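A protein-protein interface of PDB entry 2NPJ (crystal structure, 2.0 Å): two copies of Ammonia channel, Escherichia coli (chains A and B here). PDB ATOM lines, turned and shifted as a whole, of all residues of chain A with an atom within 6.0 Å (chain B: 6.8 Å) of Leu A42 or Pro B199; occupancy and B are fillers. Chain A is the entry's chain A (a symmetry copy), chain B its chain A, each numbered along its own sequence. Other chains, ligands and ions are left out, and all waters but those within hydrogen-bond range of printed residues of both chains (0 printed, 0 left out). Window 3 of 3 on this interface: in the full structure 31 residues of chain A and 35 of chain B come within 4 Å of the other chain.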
ATOM      1  N   LEU A  30      23.189   2.630  32.637  1.00  0.00           N
ATOM      2  CA  LEU A  30      22.940   3.836  33.437  1.00  0.00           C
ATOM      3  C   LEU A  30      24.085   4.826  33.289  1.00  0.00           C
ATOM      4  O   LEU A  30      23.860   6.033  33.253  1.00  0.00           O
ATOM      5  CB  LEU A  30      22.714   3.494  34.911  1.00  0.00           C
ATOM      6  CG  LEU A  30      21.422   2.711  35.214  1.00  0.00           C
ATOM      7  CD1 LEU A  30      21.375   2.337  36.709  1.00  0.00           C
ATOM      8  CD2 LEU A  30      20.182   3.499  34.799  1.00  0.00           C
ATOM      9  N   GLY A  38      19.245  13.519  26.670  1.00  0.00           N
ATOM     10  CA  GLY A  38      17.992  12.960  27.190  1.00  0.00           C
ATOM     11  C   GLY A  38      17.085  12.314  26.155  1.00  0.00           C
ATOM     12  O   GLY A  38      16.525  11.237  26.390  1.00  0.00           O
ATOM     13  N   LYS A  39      16.951  12.973  25.005  1.00  0.00           N
ATOM     14  CA  LYS A  39      16.116  12.486  23.902  1.00  0.00           C
ATOM     15  C   LYS A  39      16.599  11.159  23.294  1.00  0.00           C
ATOM     16  O   LYS A  39      15.854  10.511  22.568  1.00  0.00           O
ATOM     17  CB  LYS A  39      16.013  13.553  22.805  1.00  0.00           C
ATOM     18  CG  LYS A  39      17.290  13.732  21.982  1.00  0.00           C
ATOM     19  CD  LYS A  39      17.139  14.848  20.939  1.00  0.00           C
ATOM     20  CE  LYS A  39      18.416  14.990  20.121  1.00  0.00           C
ATOM     21  NZ  LYS A  39      18.520  16.332  19.467  1.00  0.00           N
ATOM     22  N   ASN A  40      17.836  10.765  23.582  1.00  0.00           N
ATOM     23  CA  ASN A  40      18.398   9.517  23.049  1.00  0.00           C
ATOM     24  C   ASN A  40      18.491   8.379  24.058  1.00  0.00           C
ATOM     25  O   ASN A  40      18.863   7.254  23.705  1.00  0.00           O
ATOM     26  CB  ASN A  40      19.788   9.784  22.477  1.00  0.00           C
ATOM     27  CG  ASN A  40      19.763  10.782  21.323  1.00  0.00           C
ATOM     28  OD1 ASN A  40      18.825  10.809  20.540  1.00  0.00           O
ATOM     29  ND2 ASN A  40      20.793  11.609  21.231  1.00  0.00           N
ATOM     30  N   VAL A  41      18.168   8.669  25.312  1.00  0.00           N
ATOM     31  CA  VAL A  41      18.277   7.660  26.379  1.00  0.00           C
ATOM     32  C   VAL A  41      17.459   6.384  26.146  1.00  0.00           C
ATOM     33  O   VAL A  41      18.002   5.291  26.255  1.00  0.00           O
ATOM     34  CB  VAL A  41      18.000   8.262  27.787  1.00  0.00           C
ATOM     35  CG1 VAL A  41      18.013   7.166  28.860  1.00  0.00           C
ATOM     36  CG2 VAL A  41      19.044   9.333  28.113  1.00  0.00           C
ATOM     37  N   LEU A  42      16.176   6.524  25.815  1.00  0.00           N
ATOM     38  CA  LEU A  42      15.320   5.342  25.612  1.00  0.00           C
ATOM     39  C   LEU A  42      15.838   4.397  24.530  1.00  0.00           C
ATOM     40  O   LEU A  42      15.894   3.179  24.721  1.00  0.00           O
ATOM     41  CB  LEU A  42      13.867   5.746  25.338  1.00  0.00           C
ATOM     42  CG  LEU A  42      13.135   6.546  26.425  1.00  0.00           C
ATOM     43  CD1 LEU A  42      11.646   6.694  26.087  1.00  0.00           C
ATOM     44  CD2 LEU A  42      13.326   5.923  27.811  1.00  0.00           C
ATOM     45  N   SER A  43      16.234   4.985  23.408  1.00  0.00           N
ATOM     46  CA  SER A  43      16.765   4.243  22.275  1.00  0.00           C
ATOM     47  C   SER A  43      18.051   3.506  22.655  1.00  0.00           C
ATOM     48  O   SER A  43      18.238   2.330  22.302  1.00  0.00           O
ATOM     49  CB  SER A  43      16.984   5.203  21.099  1.00  0.00           C
ATOM     50  OG  SER A  43      17.395   4.506  19.941  1.00  0.00           O
ATOM     51  N   MET A  44      18.932   4.188  23.391  1.00  0.00           N
ATOM     52  CA  MET A  44      20.176   3.583  23.817  1.00  0.00           C
ATOM     53  C   MET A  44      19.918   2.413  24.771  1.00  0.00           C
ATOM     54  O   MET A  44      20.543   1.360  24.643  1.00  0.00           O
ATOM     55  CB  MET A  44      21.099   4.630  24.459  1.00  0.00           C
ATOM     56  CG  MET A  44      22.421   4.069  25.011  1.00  0.00           C
ATOM     57  SD  MET A  44      22.303   3.375  26.675  1.00  0.00           S
ATOM     58  CE  MET A  44      21.810   4.817  27.619  1.00  0.00           C
ATOM     59  N   LEU A  45      18.988   2.588  25.715  1.00  0.00           N
ATOM     60  CA  LEU A  45      18.681   1.512  26.680  1.00  0.00           C
ATOM     61  C   LEU A  45      18.140   0.281  25.937  1.00  0.00           C
ATOM     62  O   LEU A  45      18.475  -0.850  26.289  1.00  0.00           O
ATOM     63  CB  LEU A  45      17.696   1.991  27.765  1.00  0.00           C
ATOM     64  CG  LEU A  45      18.188   3.074  28.748  1.00  0.00           C
ATOM     65  CD1 LEU A  45      17.084   3.515  29.724  1.00  0.00           C
ATOM     66  CD2 LEU A  45      19.408   2.609  29.509  1.00  0.00           C
ATOM     67  N   THR A  46      17.339   0.525  24.899  1.00  0.00           N
ATOM     68  CA  THR A  46      16.760  -0.545  24.065  1.00  0.00           C
ATOM     69  C   THR A  46      17.875  -1.293  23.317  1.00  0.00           C
ATOM     70  O   THR A  46      17.925  -2.529  23.332  1.00  0.00           O
ATOM     71  CB  THR A  46      15.712   0.001  23.090  1.00  0.00           C
ATOM     72  OG1 THR A  46      14.740   0.762  23.819  1.00  0.00           O
ATOM     73  CG2 THR A  46      14.992  -1.151  22.346  1.00  0.00           C
ATOM     74  N   GLN A  47      18.772  -0.543  22.679  1.00  0.00           N
ATOM     75  CA  GLN A  47      19.903  -1.136  21.950  1.00  0.00           C
ATOM     76  C   GLN A  47      20.830  -1.930  22.878  1.00  0.00           C
ATOM     77  O   GLN A  47      21.300  -3.016  22.519  1.00  0.00           O
ATOM     78  CB  GLN A  47      20.687  -0.055  21.207  1.00  0.00           C
ATOM     79  CG  GLN A  47      19.950   0.495  19.978  1.00  0.00           C
ATOM     80  CD  GLN A  47      20.886   1.180  19.002  1.00  0.00           C
ATOM     81  OE1 GLN A  47      22.103   1.004  19.064  1.00  0.00           O
ATOM     82  NE2 GLN A  47      20.324   1.955  18.093  1.00  0.00           N
ATOM     83  N   MET A 200      22.752   9.826  37.697  1.00  0.00           N
ATOM     84  CA  MET A 200      22.607   8.568  36.969  1.00  0.00           C
ATOM     85  C   MET A 200      24.001   8.048  36.581  1.00  0.00           C
ATOM     86  O   MET A 200      24.259   6.855  36.694  1.00  0.00           O
ATOM     87  CB  MET A 200      21.693   8.721  35.744  1.00  0.00           C
ATOM     88  CG  MET A 200      21.429   7.415  34.983  1.00  0.00           C
ATOM     89  SD  MET A 200      20.330   7.668  33.555  1.00  0.00           S
ATOM     90  CE  MET A 200      18.752   7.919  34.372  1.00  0.00           C
ATOM     91  N   GLY B  34       8.025   3.090  37.735  1.00  0.00           N
ATOM     92  CA  GLY B  34       8.142   3.789  36.454  1.00  0.00           C
ATOM     93  C   GLY B  34       6.930   3.613  35.555  1.00  0.00           C
ATOM     94  O   GLY B  34       6.774   4.339  34.572  1.00  0.00           O
ATOM     95  N   HIS B 196       5.592   6.981  32.877  1.00  0.00           N
ATOM     96  CA  HIS B 196       6.148   8.326  33.024  1.00  0.00           C
ATOM     97  C   HIS B 196       7.668   8.320  33.207  1.00  0.00           C
ATOM     98  O   HIS B 196       8.321   9.362  33.050  1.00  0.00           O
ATOM     99  CB  HIS B 196       5.486   9.039  34.211  1.00  0.00           C
ATOM    100  CG  HIS B 196       5.977   8.567  35.546  1.00  0.00           C
ATOM    101  ND1 HIS B 196       5.595   7.364  36.099  1.00  0.00           N
ATOM    102  CD2 HIS B 196       6.829   9.135  36.434  1.00  0.00           C
ATOM    103  CE1 HIS B 196       6.189   7.209  37.269  1.00  0.00           C
ATOM    104  NE2 HIS B 196       6.944   8.269  37.496  1.00  0.00           N
ATOM    105  N   ASN B 197       8.218   7.151  33.549  1.00  0.00           N
ATOM    106  CA  ASN B 197       9.645   7.002  33.791  1.00  0.00           C
ATOM    107  C   ASN B 197      10.193   5.653  33.321  1.00  0.00           C
ATOM    108  O   ASN B 197      10.421   4.757  34.127  1.00  0.00           O
ATOM    109  CB  ASN B 197       9.900   7.179  35.289  1.00  0.00           C
ATOM    110  CG  ASN B 197      11.328   7.533  35.608  1.00  0.00           C
ATOM    111  OD1 ASN B 197      12.252   7.225  34.854  1.00  0.00           O
ATOM    112  ND2 ASN B 197      11.525   8.171  36.756  1.00  0.00           N
ATOM    113  N   LEU B 198      10.426   5.517  32.020  1.00  0.00           N
ATOM    114  CA  LEU B 198      10.954   4.259  31.486  1.00  0.00           C
ATOM    115  C   LEU B 198      12.374   3.877  31.947  1.00  0.00           C
ATOM    116  O   LEU B 198      12.652   2.695  32.124  1.00  0.00           O
ATOM    117  CB  LEU B 198      10.813   4.195  29.959  1.00  0.00           C
ATOM    118  CG  LEU B 198       9.371   3.940  29.496  1.00  0.00           C
ATOM    119  CD1 LEU B 198       9.209   4.256  28.021  1.00  0.00           C
ATOM    120  CD2 LEU B 198       8.920   2.513  29.815  1.00  0.00           C
ATOM    121  N   PRO B 199      13.283   4.864  32.126  1.00  0.00           N
ATOM    122  CA  PRO B 199      14.563   4.495  32.767  1.00  0.00           C
ATOM    123  C   PRO B 199      14.391   3.800  34.129  1.00  0.00           C
ATOM    124  O   PRO B 199      15.185   2.907  34.468  1.00  0.00           O
ATOM    125  CB  PRO B 199      15.294   5.836  32.896  1.00  0.00           C
ATOM    126  CG  PRO B 199      14.737   6.660  31.763  1.00  0.00           C
ATOM    127  CD  PRO B 199      13.276   6.281  31.705  1.00  0.00           C
ATOM    128  N   MET B 200      13.365   4.186  34.889  1.00  0.00           N
ATOM    129  CA  MET B 200      13.091   3.555  36.178  1.00  0.00           C
ATOM    130  C   MET B 200      12.566   2.130  35.938  1.00  0.00           C
ATOM    131  O   MET B 200      12.963   1.209  36.642  1.00  0.00           O
ATOM    132  CB  MET B 200      12.116   4.387  37.024  1.00  0.00           C
ATOM    133  CG  MET B 200      11.852   3.822  38.426  1.00  0.00           C
ATOM    134  SD  MET B 200      10.702   4.865  39.376  1.00  0.00           S
ATOM    135  CE  MET B 200      11.745   6.273  39.758  1.00  0.00           C
ATOM    136  N   VAL B 201      11.708   1.944  34.928  1.00  0.00           N
ATOM    137  CA  VAL B 201      11.185   0.602  34.609  1.00  0.00           C
ATOM    138  C   VAL B 201      12.363  -0.307  34.227  1.00  0.00           C
ATOM    139  O   VAL B 201      12.455  -1.467  34.675  1.00  0.00           O
ATOM    140  CB  VAL B 201      10.160   0.618  33.450  1.00  0.00           C
ATOM    141  CG1 VAL B 201       9.775  -0.814  33.053  1.00  0.00           C
ATOM    142  CG2 VAL B 201       8.909   1.415  33.831  1.00  0.00           C
ATOM    143  N   PHE B 202      13.271   0.234  33.415  1.00  0.00           N
ATOM    144  CA  PHE B 202      14.461  -0.506  32.987  1.00  0.00           C
ATOM    145  C   PHE B 202      15.330  -0.892  34.201  1.00  0.00           C
ATOM    146  O   PHE B 202      15.819  -2.021  34.305  1.00  0.00           O
ATOM    147  CB  PHE B 202      15.306   0.331  32.009  1.00  0.00           C
ATOM    148  CG  PHE B 202      16.675  -0.262  31.745  1.00  0.00           C
ATOM    149  CD1 PHE B 202      16.816  -1.342  30.874  1.00  0.00           C
ATOM    150  CD2 PHE B 202      17.813   0.242  32.394  1.00  0.00           C
ATOM    151  CE1 PHE B 202      18.073  -1.920  30.639  1.00  0.00           C
ATOM    152  CE2 PHE B 202      19.083  -0.328  32.166  1.00  0.00           C
ATOM    153  CZ  PHE B 202      19.206  -1.413  31.294  1.00  0.00           C
ATOM    154  N   THR B 203      15.529   0.057  35.106  1.00  0.00           N
ATOM    155  CA  THR B 203      16.340  -0.186  36.289  1.00  0.00           C
ATOM    156  C   THR B 203      15.715  -1.295  37.143  1.00  0.00           C
ATOM    157  O   THR B 203      16.418  -2.198  37.586  1.00  0.00           O
ATOM    158  CB  THR B 203      16.580   1.103  37.089  1.00  0.00           C
ATOM    159  OG1 THR B 203      17.215   2.075  36.238  1.00  0.00           O
ATOM    160  CG2 THR B 203      17.480   0.821  38.292  1.00  0.00           C
ATOM    161  N   GLY B 204      14.394  -1.247  37.341  1.00  0.00           N
ATOM    162  CA  GLY B 204      13.701  -2.280  38.116  1.00  0.00           C
ATOM    163  C   GLY B 204      13.808  -3.634  37.430  1.00  0.00           C
ATOM    164  O   GLY B 204      13.985  -4.653  38.098  1.00  0.00           O
ATOM    165  N   SER B 257      10.690  -1.290  21.275  1.00  0.00           N
ATOM    166  CA  SER B 257      10.543  -0.214  22.255  1.00  0.00           C
ATOM    167  C   SER B 257      11.237  -0.656  23.524  1.00  0.00           C
ATOM    168  O   SER B 257      11.445  -1.853  23.731  1.00  0.00           O
ATOM    169  CB  SER B 257       9.060   0.081  22.535  1.00  0.00           C
ATOM    170  OG  SER B 257       8.493  -0.938  23.347  1.00  0.00           O
ATOM    171  N   LEU B 258      11.594   0.290  24.392  1.00  0.00           N
ATOM    172  CA  LEU B 258      12.252  -0.088  25.640  1.00  0.00           C
ATOM    173  C   LEU B 258      11.341  -0.944  26.518  1.00  0.00           C
ATOM    174  O   LEU B 258      11.793  -1.927  27.113  1.00  0.00           O
ATOM    175  CB  LEU B 258      12.722   1.146  26.425  1.00  0.00           C
ATOM    176  CG  LEU B 258      13.435   0.863  27.762  1.00  0.00           C
ATOM    177  CD1 LEU B 258      14.583  -0.145  27.602  1.00  0.00           C
ATOM    178  CD2 LEU B 258      13.933   2.172  28.375  1.00  0.00           C
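Position printed for both chains: 200.
Hydrophobic or aromatic side chains of chain B within 4 Å of the printed part of chain A: Leu B198, Pro B199, Phe B202 and Leu B258. Among the printed residues, no Asp or Glu carboxylate lies within 4 Å of a Lys or Arg side-chain nitrogen of the other chain.
Among the printed residues, merely in contact across the chains: Leu A30 with Thr B203, Leu A45 with Leu B258, Leu A42 with Leu B198, Thr A46 with Ser B257, Leu A42 with Leu B258, Leu A42 with Pro B199 and Leu A45 with Phe B202.
OG1 of Thr B203 is in hydrogen-bond range of O of Pro B199. O of Leu A42 sits at hydrogen-bond distance from OG1 of Thr A46.
Leu A42 touches just these residues of chain B: Leu B198 (3.7 Å), Pro B199 (3.9 Å) and Leu B258 (3.8 Å). Printed residues of chain A within 4 Å of Leu B198: Leu A42. Of the printed residues of chain B, Leu A45 touches Phe B202 and Leu B258. Met B200 touches none of the printed residues of chain A.
The backbone NH (N) of Leu B258 sits close to the side-chain hydroxyl (OG1) of Thr A46, 3.2 Å away.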
